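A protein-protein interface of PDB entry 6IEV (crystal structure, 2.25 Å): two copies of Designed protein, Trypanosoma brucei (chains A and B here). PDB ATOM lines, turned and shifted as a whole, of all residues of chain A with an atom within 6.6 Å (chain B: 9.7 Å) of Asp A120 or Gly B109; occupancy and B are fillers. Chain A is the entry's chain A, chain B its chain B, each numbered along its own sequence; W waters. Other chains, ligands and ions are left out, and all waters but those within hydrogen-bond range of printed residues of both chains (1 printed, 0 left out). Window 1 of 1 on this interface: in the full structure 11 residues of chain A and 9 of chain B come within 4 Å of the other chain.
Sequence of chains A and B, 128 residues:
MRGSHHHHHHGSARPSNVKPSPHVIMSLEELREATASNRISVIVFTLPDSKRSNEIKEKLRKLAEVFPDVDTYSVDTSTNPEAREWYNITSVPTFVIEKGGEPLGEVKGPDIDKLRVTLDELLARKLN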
ATOM      1  N   PHE A  67     -33.499   3.442  19.136  1.00  0.00           N
ATOM      2  CA  PHE A  67     -32.784   3.768  17.916  1.00  0.00           C
ATOM      3  C   PHE A  67     -33.273   5.108  17.401  1.00  0.00           C
ATOM      4  O   PHE A  67     -34.442   5.235  16.998  1.00  0.00           O
ATOM      5  CB  PHE A  67     -32.952   2.675  16.862  1.00  0.00           C
ATOM      6  CG  PHE A  67     -32.096   1.468  17.119  1.00  0.00           C
ATOM      7  CD1 PHE A  67     -30.775   1.452  16.733  1.00  0.00           C
ATOM      8  CD2 PHE A  67     -32.607   0.364  17.784  1.00  0.00           C
ATOM      9  CE1 PHE A  67     -29.988   0.348  16.981  1.00  0.00           C
ATOM     10  CE2 PHE A  67     -31.827  -0.741  18.029  1.00  0.00           C
ATOM     11  CZ  PHE A  67     -30.522  -0.750  17.628  1.00  0.00           C
ATOM     12  N   LEU A 115     -34.370  -9.631  14.292  1.00  0.00           N
ATOM     13  CA  LEU A 115     -34.529  -8.341  13.651  1.00  0.00           C
ATOM     14  C   LEU A 115     -33.565  -7.325  14.239  1.00  0.00           C
ATOM     15  O   LEU A 115     -32.846  -6.643  13.501  1.00  0.00           O
ATOM     16  CB  LEU A 115     -35.978  -7.866  13.767  1.00  0.00           C
ATOM     17  CG  LEU A 115     -35.977  -6.469  13.179  1.00  0.00           C
ATOM     18  CD1 LEU A 115     -35.748  -6.526  11.658  1.00  0.00           C
ATOM     19  CD2 LEU A 115     -37.225  -5.693  13.516  1.00  0.00           C
ATOM     20  N   ARG A 116     -33.503  -7.240  15.570  1.00  0.00           N
ATOM     21  CA  ARG A 116     -32.554  -6.317  16.196  1.00  0.00           C
ATOM     22  C   ARG A 116     -31.114  -6.657  15.813  1.00  0.00           C
ATOM     23  O   ARG A 116     -30.319  -5.762  15.494  1.00  0.00           O
ATOM     24  CB  ARG A 116     -32.745  -6.313  17.710  1.00  0.00           C
ATOM     25  CG  ARG A 116     -31.985  -5.178  18.377  1.00  0.00           C
ATOM     26  CD  ARG A 116     -32.372  -5.052  19.825  1.00  0.00           C
ATOM     27  NE  ARG A 116     -31.657  -3.947  20.462  1.00  0.00           N
ATOM     28  CZ  ARG A 116     -31.967  -3.438  21.651  1.00  0.00           C
ATOM     29  NH1 ARG A 116     -32.989  -3.919  22.346  1.00  0.00           N
ATOM     30  NH2 ARG A 116     -31.248  -2.441  22.145  1.00  0.00           N
ATOM     31  N   VAL A 117     -30.761  -7.947  15.822  1.00  0.00           N
ATOM     32  CA  VAL A 117     -29.407  -8.351  15.436  1.00  0.00           C
ATOM     33  C   VAL A 117     -29.115  -7.926  14.007  1.00  0.00           C
ATOM     34  O   VAL A 117     -28.059  -7.353  13.708  1.00  0.00           O
ATOM     35  CB  VAL A 117     -29.225  -9.865  15.620  1.00  0.00           C
ATOM     36  CG1 VAL A 117     -27.896 -10.295  15.052  1.00  0.00           C
ATOM     37  CG2 VAL A 117     -29.337 -10.236  17.089  1.00  0.00           C
ATOM     38  N   THR A 118     -30.059  -8.189  13.102  1.00  0.00           N
ATOM     39  CA  THR A 118     -29.873  -7.819  11.703  1.00  0.00           C
ATOM     40  C   THR A 118     -29.700  -6.318  11.558  1.00  0.00           C
ATOM     41  O   THR A 118     -28.847  -5.844  10.792  1.00  0.00           O
ATOM     42  CB  THR A 118     -31.078  -8.278  10.878  1.00  0.00           C
ATOM     43  OG1 THR A 118     -31.287  -9.679  11.073  1.00  0.00           O
ATOM     44  CG2 THR A 118     -30.870  -7.965   9.400  1.00  0.00           C
ATOM     45  N   LEU A 119     -30.522  -5.549  12.277  1.00  0.00           N
ATOM     46  CA  LEU A 119     -30.443  -4.098  12.193  1.00  0.00           C
ATOM     47  C   LEU A 119     -29.106  -3.601  12.718  1.00  0.00           C
ATOM     48  O   LEU A 119     -28.481  -2.726  12.108  1.00  0.00           O
ATOM     49  CB  LEU A 119     -31.611  -3.468  12.957  1.00  0.00           C
ATOM     50  CG  LEU A 119     -31.538  -1.945  13.081  1.00  0.00           C
ATOM     51  CD1 LEU A 119     -31.478  -1.311  11.696  1.00  0.00           C
ATOM     52  CD2 LEU A 119     -32.685  -1.396  13.940  1.00  0.00           C
ATOM     53  N   ASP A 120     -28.633  -4.172  13.832  1.00  0.00           N
ATOM     54  CA  ASP A 120     -27.341  -3.754  14.379  1.00  0.00           C
ATOM     55  C   ASP A 120     -26.219  -3.996  13.375  1.00  0.00           C
ATOM     56  O   ASP A 120     -25.339  -3.143  13.187  1.00  0.00           O
ATOM     57  CB  ASP A 120     -27.058  -4.506  15.683  1.00  0.00           C
ATOM     58  CG  ASP A 120     -27.817  -3.940  16.867  1.00  0.00           C
ATOM     59  OD1 ASP A 120     -28.150  -2.735  16.841  1.00  0.00           O
ATOM     60  OD2 ASP A 120     -28.060  -4.697  17.831  1.00  0.00           O
ATOM     61  N   GLU A 121     -26.271  -5.134  12.685  1.00  0.00           N
ATOM     62  CA  GLU A 121     -25.266  -5.464  11.685  1.00  0.00           C
ATOM     63  C   GLU A 121     -25.346  -4.526  10.484  1.00  0.00           C
ATOM     64  O   GLU A 121     -24.318  -4.198   9.878  1.00  0.00           O
ATOM     65  CB  GLU A 121     -25.469  -6.918  11.271  1.00  0.00           C
ATOM     66  CG  GLU A 121     -24.370  -7.559  10.476  1.00  0.00           C
ATOM     67  CD  GLU A 121     -24.921  -8.579   9.494  1.00  0.00           C
ATOM     68  OE1 GLU A 121     -24.124  -9.398   8.987  1.00  0.00           O
ATOM     69  OE2 GLU A 121     -26.144  -8.551   9.209  1.00  0.00           O
ATOM     70  N   LEU A 122     -26.546  -4.044  10.145  1.00  0.00           N
ATOM     71  CA  LEU A 122     -26.643  -3.055   9.076  1.00  0.00           C
ATOM     72  C   LEU A 122     -26.069  -1.714   9.496  1.00  0.00           C
ATOM     73  O   LEU A 122     -25.458  -1.025   8.675  1.00  0.00           O
ATOM     74  CB  LEU A 122     -28.092  -2.905   8.626  1.00  0.00           C
ATOM     75  CG  LEU A 122     -28.499  -4.166   7.873  1.00  0.00           C
ATOM     76  CD1 LEU A 122     -29.994  -4.359   7.900  1.00  0.00           C
ATOM     77  CD2 LEU A 122     -27.967  -4.100   6.455  1.00  0.00           C
ATOM     78  N   LEU A 123     -26.249  -1.324  10.763  1.00  0.00           N
ATOM     79  CA  LEU A 123     -25.665  -0.068  11.230  1.00  0.00           C
ATOM     80  C   LEU A 123     -24.162  -0.169  11.435  1.00  0.00           C
ATOM     81  O   LEU A 123     -23.491   0.861  11.460  1.00  0.00           O
ATOM     82  CB  LEU A 123     -26.291   0.355  12.559  1.00  0.00           C
ATOM     83  CG  LEU A 123     -27.803   0.569  12.527  1.00  0.00           C
ATOM     84  CD1 LEU A 123     -28.317   0.910  13.914  1.00  0.00           C
ATOM     85  CD2 LEU A 123     -28.112   1.670  11.530  1.00  0.00           C
ATOM     86  N   ALA A 124     -23.615  -1.377  11.486  1.00  0.00           N
ATOM     87  CA  ALA A 124     -22.188  -1.544  11.692  1.00  0.00           C
ATOM     88  C   ALA A 124     -21.428  -1.289  10.395  1.00  0.00           C
ATOM     89  O   ALA A 124     -22.010  -1.150   9.322  1.00  0.00           O
ATOM     90  CB  ALA A 124     -21.900  -2.952  12.214  1.00  0.00           C
ATOM     91  N   ARG A 125     -20.107  -1.219  10.505  1.00  0.00           N
ATOM     92  CA  ARG A 125     -19.230  -1.100   9.350  1.00  0.00           C
ATOM     93  C   ARG A 125     -18.537  -2.445   9.144  1.00  0.00           C
ATOM     94  O   ARG A 125     -17.812  -2.904  10.033  1.00  0.00           O
ATOM     95  CB  ARG A 125     -18.207   0.020   9.553  1.00  0.00           C
ATOM     96  CG  ARG A 125     -17.491   0.467   8.284  1.00  0.00           C
ATOM     97  CD  ARG A 125     -16.310   1.408   8.567  1.00  0.00           C
ATOM     98  NE  ARG A 125     -16.557   2.771   8.091  1.00  0.00           N
ATOM     99  CZ  ARG A 125     -16.115   3.260   6.930  1.00  0.00           C
ATOM    100  NH1 ARG A 125     -15.394   2.498   6.113  1.00  0.00           N
ATOM    101  NH2 ARG A 125     -16.396   4.512   6.577  1.00  0.00           N
ATOM    102  N   ILE B  43     -15.095  -5.317  26.136  1.00  0.00           N
ATOM    103  CA  ILE B  43     -14.118  -4.929  25.126  1.00  0.00           C
ATOM    104  C   ILE B  43     -14.865  -4.452  23.888  1.00  0.00           C
ATOM    105  O   ILE B  43     -15.710  -5.179  23.363  1.00  0.00           O
ATOM    106  CB  ILE B  43     -13.215  -6.126  24.771  1.00  0.00           C
ATOM    107  CG1 ILE B  43     -12.662  -6.761  26.038  1.00  0.00           C
ATOM    108  CG2 ILE B  43     -12.159  -5.778  23.731  1.00  0.00           C
ATOM    109  CD1 ILE B  43     -12.633  -8.271  25.964  1.00  0.00           C
ATOM    110  N   VAL B  44     -14.555  -3.251  23.410  1.00  0.00           N
ATOM    111  CA  VAL B  44     -15.103  -2.768  22.150  1.00  0.00           C
ATOM    112  C   VAL B  44     -14.024  -2.834  21.074  1.00  0.00           C
ATOM    113  O   VAL B  44     -12.904  -2.346  21.269  1.00  0.00           O
ATOM    114  CB  VAL B  44     -15.712  -1.359  22.267  1.00  0.00           C
ATOM    115  CG1 VAL B  44     -14.663  -0.301  22.490  1.00  0.00           C
ATOM    116  CG2 VAL B  44     -16.513  -1.042  20.982  1.00  0.00           C
ATOM    117  N   PHE B  45     -14.365  -3.462  19.948  1.00  0.00           N
ATOM    118  CA  PHE B  45     -13.507  -3.547  18.769  1.00  0.00           C
ATOM    119  C   PHE B  45     -13.963  -2.487  17.770  1.00  0.00           C
ATOM    120  O   PHE B  45     -15.123  -2.487  17.362  1.00  0.00           O
ATOM    121  CB  PHE B  45     -13.583  -4.947  18.155  1.00  0.00           C
ATOM    122  CG  PHE B  45     -12.998  -6.032  19.043  1.00  0.00           C
ATOM    123  CD1 PHE B  45     -13.759  -6.607  20.051  1.00  0.00           C
ATOM    124  CD2 PHE B  45     -11.686  -6.464  18.866  1.00  0.00           C
ATOM    125  CE1 PHE B  45     -13.225  -7.594  20.876  1.00  0.00           C
ATOM    126  CE2 PHE B  45     -11.132  -7.436  19.699  1.00  0.00           C
ATOM    127  CZ  PHE B  45     -11.890  -8.011  20.702  1.00  0.00           C
ATOM    128  N   THR B  46     -13.074  -1.557  17.420  1.00  0.00           N
ATOM    129  CA  THR B  46     -13.425  -0.403  16.598  1.00  0.00           C
ATOM    130  C   THR B  46     -12.390  -0.204  15.507  1.00  0.00           C
ATOM    131  O   THR B  46     -11.310  -0.802  15.525  1.00  0.00           O
ATOM    132  CB  THR B  46     -13.491   0.901  17.411  1.00  0.00           C
ATOM    133  OG1 THR B  46     -12.170   1.250  17.841  1.00  0.00           O
ATOM    134  CG2 THR B  46     -14.354   0.754  18.621  1.00  0.00           C
ATOM    135  N   ILE B  56     -18.535   5.864  20.455  1.00  0.00           N
ATOM    136  CA  ILE B  56     -18.876   4.608  21.116  1.00  0.00           C
ATOM    137  C   ILE B  56     -17.975   4.373  22.330  1.00  0.00           C
ATOM    138  O   ILE B  56     -18.426   3.817  23.337  1.00  0.00           O
ATOM    139  CB  ILE B  56     -18.852   3.431  20.123  1.00  0.00           C
ATOM    140  CG1 ILE B  56     -19.802   2.329  20.601  1.00  0.00           C
ATOM    141  CG2 ILE B  56     -17.441   2.886  19.961  1.00  0.00           C
ATOM    142  CD1 ILE B  56     -21.272   2.532  20.190  1.00  0.00           C
ATOM    143  N   LYS B  59     -19.512   6.136  25.244  1.00  0.00           N
ATOM    144  CA  LYS B  59     -20.661   5.354  25.685  1.00  0.00           C
ATOM    145  C   LYS B  59     -20.225   4.175  26.539  1.00  0.00           C
ATOM    146  O   LYS B  59     -20.866   3.865  27.548  1.00  0.00           O
ATOM    147  CB  LYS B  59     -21.476   4.875  24.480  1.00  0.00           C
ATOM    148  CG  LYS B  59     -22.470   5.914  23.967  1.00  0.00           C
ATOM    149  CD  LYS B  59     -23.134   5.457  22.657  1.00  0.00           C
ATOM    150  CE  LYS B  59     -24.131   6.493  22.154  1.00  0.00           C
ATOM    151  NZ  LYS B  59     -24.957   5.996  21.019  1.00  0.00           N
ATOM    152  N   ILE B  89     -13.896 -10.988  14.798  1.00  0.00           N
ATOM    153  CA  ILE B  89     -14.500  -9.674  14.583  1.00  0.00           C
ATOM    154  C   ILE B  89     -14.659  -9.443  13.084  1.00  0.00           C
ATOM    155  O   ILE B  89     -13.673  -9.427  12.347  1.00  0.00           O
ATOM    156  CB  ILE B  89     -13.670  -8.547  15.215  1.00  0.00           C
ATOM    157  CG1 ILE B  89     -13.412  -8.786  16.715  1.00  0.00           C
ATOM    158  CG2 ILE B  89     -14.352  -7.190  14.969  1.00  0.00           C
ATOM    159  CD1 ILE B  89     -14.683  -9.046  17.596  1.00  0.00           C
ATOM    160  N   THR B  90     -15.901  -9.325  12.617  1.00  0.00           N
ATOM    161  CA  THR B  90     -16.165  -9.068  11.200  1.00  0.00           C
ATOM    162  C   THR B  90     -16.782  -7.700  10.939  1.00  0.00           C
ATOM    163  O   THR B  90     -16.771  -7.236   9.794  1.00  0.00           O
ATOM    164  CB  THR B  90     -17.071 -10.153  10.596  1.00  0.00           C
ATOM    165  OG1 THR B  90     -18.256 -10.295  11.382  1.00  0.00           O
ATOM    166  CG2 THR B  90     -16.333 -11.490  10.534  1.00  0.00           C
ATOM    167  N   SER B  91     -17.303  -7.038  11.966  1.00  0.00           N
ATOM    168  CA  SER B  91     -17.812  -5.690  11.817  1.00  0.00           C
ATOM    169  C   SER B  91     -17.501  -4.926  13.087  1.00  0.00           C
ATOM    170  O   SER B  91     -17.362  -5.512  14.163  1.00  0.00           O
ATOM    171  CB  SER B  91     -19.337  -5.689  11.566  1.00  0.00           C
ATOM    172  OG  SER B  91     -19.666  -6.321  10.331  1.00  0.00           O
ATOM    173  N   VAL B  92     -17.416  -3.608  12.954  1.00  0.00           N
ATOM    174  CA  VAL B  92     -17.151  -2.733  14.086  1.00  0.00           C
ATOM    175  C   VAL B  92     -18.269  -1.704  14.174  1.00  0.00           C
ATOM    176  O   VAL B  92     -18.866  -1.351  13.151  1.00  0.00           O
ATOM    177  CB  VAL B  92     -15.778  -2.067  13.943  1.00  0.00           C
ATOM    178  CG1 VAL B  92     -14.707  -3.127  13.909  1.00  0.00           C
ATOM    179  CG2 VAL B  92     -15.744  -1.262  12.669  1.00  0.00           C
ATOM    180  N   PRO B  93     -18.622  -1.236  15.367  1.00  0.00           N
ATOM    181  CA  PRO B  93     -18.077  -1.787  16.613  1.00  0.00           C
ATOM    182  C   PRO B  93     -18.741  -3.102  17.019  1.00  0.00           C
ATOM    183  O   PRO B  93     -19.916  -3.337  16.760  1.00  0.00           O
ATOM    184  CB  PRO B  93     -18.372  -0.699  17.645  1.00  0.00           C
ATOM    185  CG  PRO B  93     -19.624   0.007  17.086  1.00  0.00           C
ATOM    186  CD  PRO B  93     -19.456  -0.040  15.586  1.00  0.00           C
ATOM    187  N   THR B  94     -17.968  -3.946  17.680  1.00  0.00           N
ATOM    188  CA  THR B  94     -18.476  -5.161  18.293  1.00  0.00           C
ATOM    189  C   THR B  94     -17.990  -5.156  19.734  1.00  0.00           C
ATOM    190  O   THR B  94     -16.827  -4.858  19.983  1.00  0.00           O
ATOM    191  CB  THR B  94     -17.959  -6.419  17.568  1.00  0.00           C
ATOM    192  OG1 THR B  94     -18.451  -6.446  16.213  1.00  0.00           O
ATOM    193  CG2 THR B  94     -18.369  -7.694  18.325  1.00  0.00           C
ATOM    194  N   PHE B  95     -18.877  -5.504  20.664  1.00  0.00           N
ATOM    195  CA  PHE B  95     -18.577  -5.643  22.079  1.00  0.00           C
ATOM    196  C   PHE B  95     -18.519  -7.113  22.448  1.00  0.00           C
ATOM    197  O   PHE B  95     -19.354  -7.905  22.006  1.00  0.00           O
ATOM    198  CB  PHE B  95     -19.639  -4.971  22.954  1.00  0.00           C
ATOM    199  CG  PHE B  95     -19.891  -3.550  22.600  1.00  0.00           C
ATOM    200  CD1 PHE B  95     -20.795  -3.219  21.594  1.00  0.00           C
ATOM    201  CD2 PHE B  95     -19.214  -2.536  23.255  1.00  0.00           C
ATOM    202  CE1 PHE B  95     -21.025  -1.894  21.258  1.00  0.00           C
ATOM    203  CE2 PHE B  95     -19.427  -1.211  22.918  1.00  0.00           C
ATOM    204  CZ  PHE B  95     -20.337  -0.889  21.927  1.00  0.00           C
ATOM    205  N   VAL B  96     -17.524  -7.472  23.254  1.00  0.00           N
ATOM    206  CA  VAL B  96     -17.391  -8.807  23.805  1.00  0.00           C
ATOM    207  C   VAL B  96     -17.310  -8.683  25.319  1.00  0.00           C
ATOM    208  O   VAL B  96     -16.571  -7.835  25.835  1.00  0.00           O
ATOM    209  CB  VAL B  96     -16.147  -9.524  23.246  1.00  0.00           C
ATOM    210  CG1 VAL B  96     -16.015 -10.874  23.899  1.00  0.00           C
ATOM    211  CG2 VAL B  96     -16.261  -9.668  21.726  1.00  0.00           C
ATOM    212  N   GLU B 106     -21.832 -11.231  23.439  1.00  0.00           N
ATOM    213  CA  GLU B 106     -21.291 -10.506  22.304  1.00  0.00           C
ATOM    214  C   GLU B 106     -22.415  -9.663  21.745  1.00  0.00           C
ATOM    215  O   GLU B 106     -23.565 -10.097  21.745  1.00  0.00           O
ATOM    216  CB  GLU B 106     -20.759 -11.488  21.247  1.00  0.00           C
ATOM    217  CG  GLU B 106     -20.269 -10.901  19.945  1.00  0.00           C
ATOM    218  CD  GLU B 106     -19.557 -11.953  19.091  1.00  0.00           C
ATOM    219  OE1 GLU B 106     -20.245 -12.878  18.600  1.00  0.00           O
ATOM    220  OE2 GLU B 106     -18.317 -11.871  18.919  1.00  0.00           O
ATOM    221  N   VAL B 107     -22.099  -8.447  21.337  1.00  0.00           N
ATOM    222  CA  VAL B 107     -23.058  -7.585  20.669  1.00  0.00           C
ATOM    223  C   VAL B 107     -22.375  -7.022  19.437  1.00  0.00           C
ATOM    224  O   VAL B 107     -21.351  -6.338  19.551  1.00  0.00           O
ATOM    225  CB  VAL B 107     -23.573  -6.464  21.584  1.00  0.00           C
ATOM    226  CG1 VAL B 107     -24.251  -5.402  20.755  1.00  0.00           C
ATOM    227  CG2 VAL B 107     -24.517  -7.040  22.603  1.00  0.00           C
ATOM    228  N   LYS B 108     -22.903  -7.355  18.264  1.00  0.00           N
ATOM    229  CA  LYS B 108     -22.310  -6.947  17.006  1.00  0.00           C
ATOM    230  C   LYS B 108     -23.045  -5.693  16.549  1.00  0.00           C
ATOM    231  O   LYS B 108     -24.252  -5.740  16.318  1.00  0.00           O
ATOM    232  CB  LYS B 108     -22.452  -8.079  15.991  1.00  0.00           C
ATOM    233  CG  LYS B 108     -21.439  -8.086  14.874  1.00  0.00           C
ATOM    234  CD  LYS B 108     -21.889  -9.041  13.792  1.00  0.00           C
ATOM    235  CE  LYS B 108     -20.958  -9.028  12.605  1.00  0.00           C
ATOM    236  NZ  LYS B 108     -21.384 -10.069  11.628  1.00  0.00           N
ATOM    237  N   GLY B 109     -22.324  -4.587  16.389  1.00  0.00           N
ATOM    238  CA  GLY B 109     -22.945  -3.348  15.980  1.00  0.00           C
ATOM    239  C   GLY B 109     -23.085  -2.355  17.117  1.00  0.00           C
ATOM    240  O   GLY B 109     -22.916  -2.689  18.295  1.00  0.00           O
ATOM    241  N   PRO B 110     -23.462  -1.108  16.799  1.00  0.00           N
ATOM    242  CA  PRO B 110     -23.484  -0.012  17.757  1.00  0.00           C
ATOM    243  C   PRO B 110     -24.723   0.069  18.656  1.00  0.00           C
ATOM    244  O   PRO B 110     -25.420   1.078  18.686  1.00  0.00           O
ATOM    245  CB  PRO B 110     -23.370   1.231  16.874  1.00  0.00           C
ATOM    246  CG  PRO B 110     -23.954   0.821  15.565  1.00  0.00           C
ATOM    247  CD  PRO B 110     -23.758  -0.664  15.420  1.00  0.00           C
ATOM    248  N   ASP B 111     -25.052  -1.041  19.313  1.00  0.00           N
ATOM    249  CA  ASP B 111     -26.231  -1.131  20.178  1.00  0.00           C
ATOM    250  C   ASP B 111     -25.794  -1.148  21.647  1.00  0.00           C
ATOM    251  O   ASP B 111     -25.782  -2.200  22.305  1.00  0.00           O
ATOM    252  CB  ASP B 111     -27.039  -2.396  19.800  1.00  0.00           C
ATOM    253  CG  ASP B 111     -28.472  -2.353  20.291  1.00  0.00           C
ATOM    254  OD1 ASP B 111     -28.795  -1.470  21.108  1.00  0.00           O
ATOM    255  OD2 ASP B 111     -29.288  -3.195  19.826  1.00  0.00           O
ATOM    256  N   ILE B 112     -25.508   0.039  22.198  1.00  0.00           N
ATOM    257  CA  ILE B 112     -25.073   0.077  23.591  1.00  0.00           C
ATOM    258  C   ILE B 112     -26.203  -0.379  24.495  1.00  0.00           C
ATOM    259  O   ILE B 112     -25.963  -0.942  25.578  1.00  0.00           O
ATOM    260  CB  ILE B 112     -24.534   1.467  23.998  1.00  0.00           C
ATOM    261  CG1 ILE B 112     -23.686   1.321  25.252  1.00  0.00           C
ATOM    262  CG2 ILE B 112     -25.644   2.437  24.325  1.00  0.00           C
ATOM    263  CD1 ILE B 112     -22.256   0.902  24.965  1.00  0.00           C
ATOM    264  N   ASP B 113     -27.455  -0.190  24.069  1.00  0.00           N
ATOM    265  CA  ASP B 113     -28.547  -0.569  24.951  1.00  0.00           C
ATOM    266  C   ASP B 113     -28.650  -2.083  25.076  1.00  0.00           C
ATOM    267  O   ASP B 113     -28.857  -2.600  26.175  1.00  0.00           O
ATOM    268  CB  ASP B 113     -29.872   0.008  24.445  1.00  0.00           C
ATOM    269  CG  ASP B 113     -31.079  -0.546  25.206  1.00  0.00           C
ATOM    270  OD1 ASP B 113     -31.381  -0.022  26.305  1.00  0.00           O
ATOM    271  OD2 ASP B 113     -31.705  -1.523  24.718  1.00  0.00           O
ATOM    272  N   LYS B 114     -28.392  -2.828  23.991  1.00  0.00           N
ATOM    273  CA  LYS B 114     -28.431  -4.281  24.125  1.00  0.00           C
ATOM    274  C   LYS B 114     -27.266  -4.796  24.952  1.00  0.00           C
ATOM    275  O   LYS B 114     -27.419  -5.764  25.712  1.00  0.00           O
ATOM    276  CB  LYS B 114     -28.439  -4.959  22.753  1.00  0.00           C
ATOM    277  CG  LYS B 114     -28.621  -6.453  22.860  1.00  0.00           C
ATOM    278  CD  LYS B 114     -28.108  -7.163  21.634  1.00  0.00           C
ATOM    279  CE  LYS B 114     -29.249  -7.815  20.877  1.00  0.00           C
ATOM    280  NZ  LYS B 114     -29.368  -9.256  21.226  1.00  0.00           N
ATOM    281  N   LEU B 115     -26.119  -4.120  24.878  1.00  0.00           N
ATOM    282  CA  LEU B 115     -25.005  -4.484  25.752  1.00  0.00           C
ATOM    283  C   LEU B 115     -25.389  -4.298  27.214  1.00  0.00           C
ATOM    284  O   LEU B 115     -25.108  -5.163  28.062  1.00  0.00           O
ATOM    285  CB  LEU B 115     -23.765  -3.651  25.407  1.00  0.00           C
ATOM    286  CG  LEU B 115     -22.557  -3.779  26.347  1.00  0.00           C
ATOM    287  CD1 LEU B 115     -21.976  -5.202  26.301  1.00  0.00           C
ATOM    288  CD2 LEU B 115     -21.502  -2.786  25.930  1.00  0.00           C
ATOM    289  N   THR B 118     -27.738  -7.142  28.182  1.00  0.00           N
ATOM    290  CA  THR B 118     -27.011  -8.405  28.330  1.00  0.00           C
ATOM    291  C   THR B 118     -26.241  -8.441  29.650  1.00  0.00           C
ATOM    292  O   THR B 118     -26.231  -9.458  30.352  1.00  0.00           O
ATOM    293  CB  THR B 118     -26.045  -8.586  27.153  1.00  0.00           C
ATOM    294  OG1 THR B 118     -26.763  -8.531  25.918  1.00  0.00           O
ATOM    295  CG2 THR B 118     -25.316  -9.909  27.237  1.00  0.00           C
HETATM  296  O   HOH W   1     -25.685  -8.074  15.030  1.00  0.00           O
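NE of Arg A116 is in salt-bridge range of OD2 of Asp B111 (2.6 Å).
The side-chain carboxylate (OD2) of Asp B113 lies within salt-bridge range of the guanidinium group (NH2) of Arg A116 (2.8 Å).
The side-chain carboxylate of Glu A121 lies within salt-bridge range of the side-chain amino group of Lys B108, 3.9 Å away.
The backbone NH (N) of Arg A125 sits at hydrogen-bond distance from the backbone carbonyl oxygen (O) of Val B92 (2.9 Å).
NH2 of Arg A116 lies close to N of Lys B114, at 3.4 Å.
OD2 of Asp A120 lies close to OD2 of Asp B111, at 2.8 Å.
The side-chain hydroxyl of Thr B90 sits at hydrogen-bond distance from the side-chain amino group of Lys B108.
O of Ser B91 is in hydrogen-bond range of OG1 of Thr B94 (2.5 Å).
O of Pro B93 is in hydrogen-bond range of N of Gly B109, at 2.7 Å.
The side-chain carboxylate (OD1) of Asp B111 sits close to the backbone NH (N) of Asp B113, 3.5 Å away.
OD1 of Asp B111 lies within hydrogen-bond range of N of Lys B114 (3.2 Å).
O of Lys B114 is in hydrogen-bond range of OG1 of Thr B118, at 2.9 Å.
Among the printed residues, merely in contact across the chains: Asp A120 with Lys B108 (3.1 Å), Arg A125 with Ser B91 (3.3 Å), Phe A67 with Asp B111 (3.5 Å), Ala A124 with Val B92 (3.6 Å), Asp A120 with Gly B109 (3.7 Å), Asp A120 with Pro B110 (3.7 Å), Ala A124 with Ser B91 (3.8 Å), Leu A123 with Pro B110 (3.8 Å) and Ala A124 with Gly B109 (3.9 Å).
Of the printed residues of chain B, Phe A67 touches Asp B111 (3.5 Å).
No residue of chain B comes within 4 Å of Leu A119.
Printed residues of chain B within 4 Å of Ala A124: Ser B91, Val B92 and Gly B109.
Of the printed residues of chain A, Val B92 touches Ala A124 (3.6 Å) and Arg A125 (2.9 Å).
Of chain A, only Asp A120 (3.7 Å) and Ala A124 (3.9 Å) come within 4 Å of Gly B109.
Of the printed residues of chain A, Lys B114 touches Arg A116 (3.4 Å).
The nearest residue of chain B that does not touch Asp A120 is Lys B114 (4.5 Å).
Of the 12 printed residues of chain A, 7 touch a printed residue of chain B.
Hydrophobic or aromatic side chains of chain A within 4 Å of the printed part of chain B: Phe A67, Leu A123 and Ala A124.
Printed residues of chain B that touch a printed residue of chain A: Ser B91, Val B92, Lys B108, Gly B109, Pro B110, Asp B111, Asp B113 and Lys B114.
Positions printed for both chains: 115 and 118.
Of the 15 pairs that touch across the chains among the printed residues, none has its exchanged pair printed and touching as well.
Water W1 bridges the backbone carbonyl oxygen (O) of Val A117 (2.8 Å) and the backbone carbonyl oxygen (O) of Lys B108 (3.0 Å).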
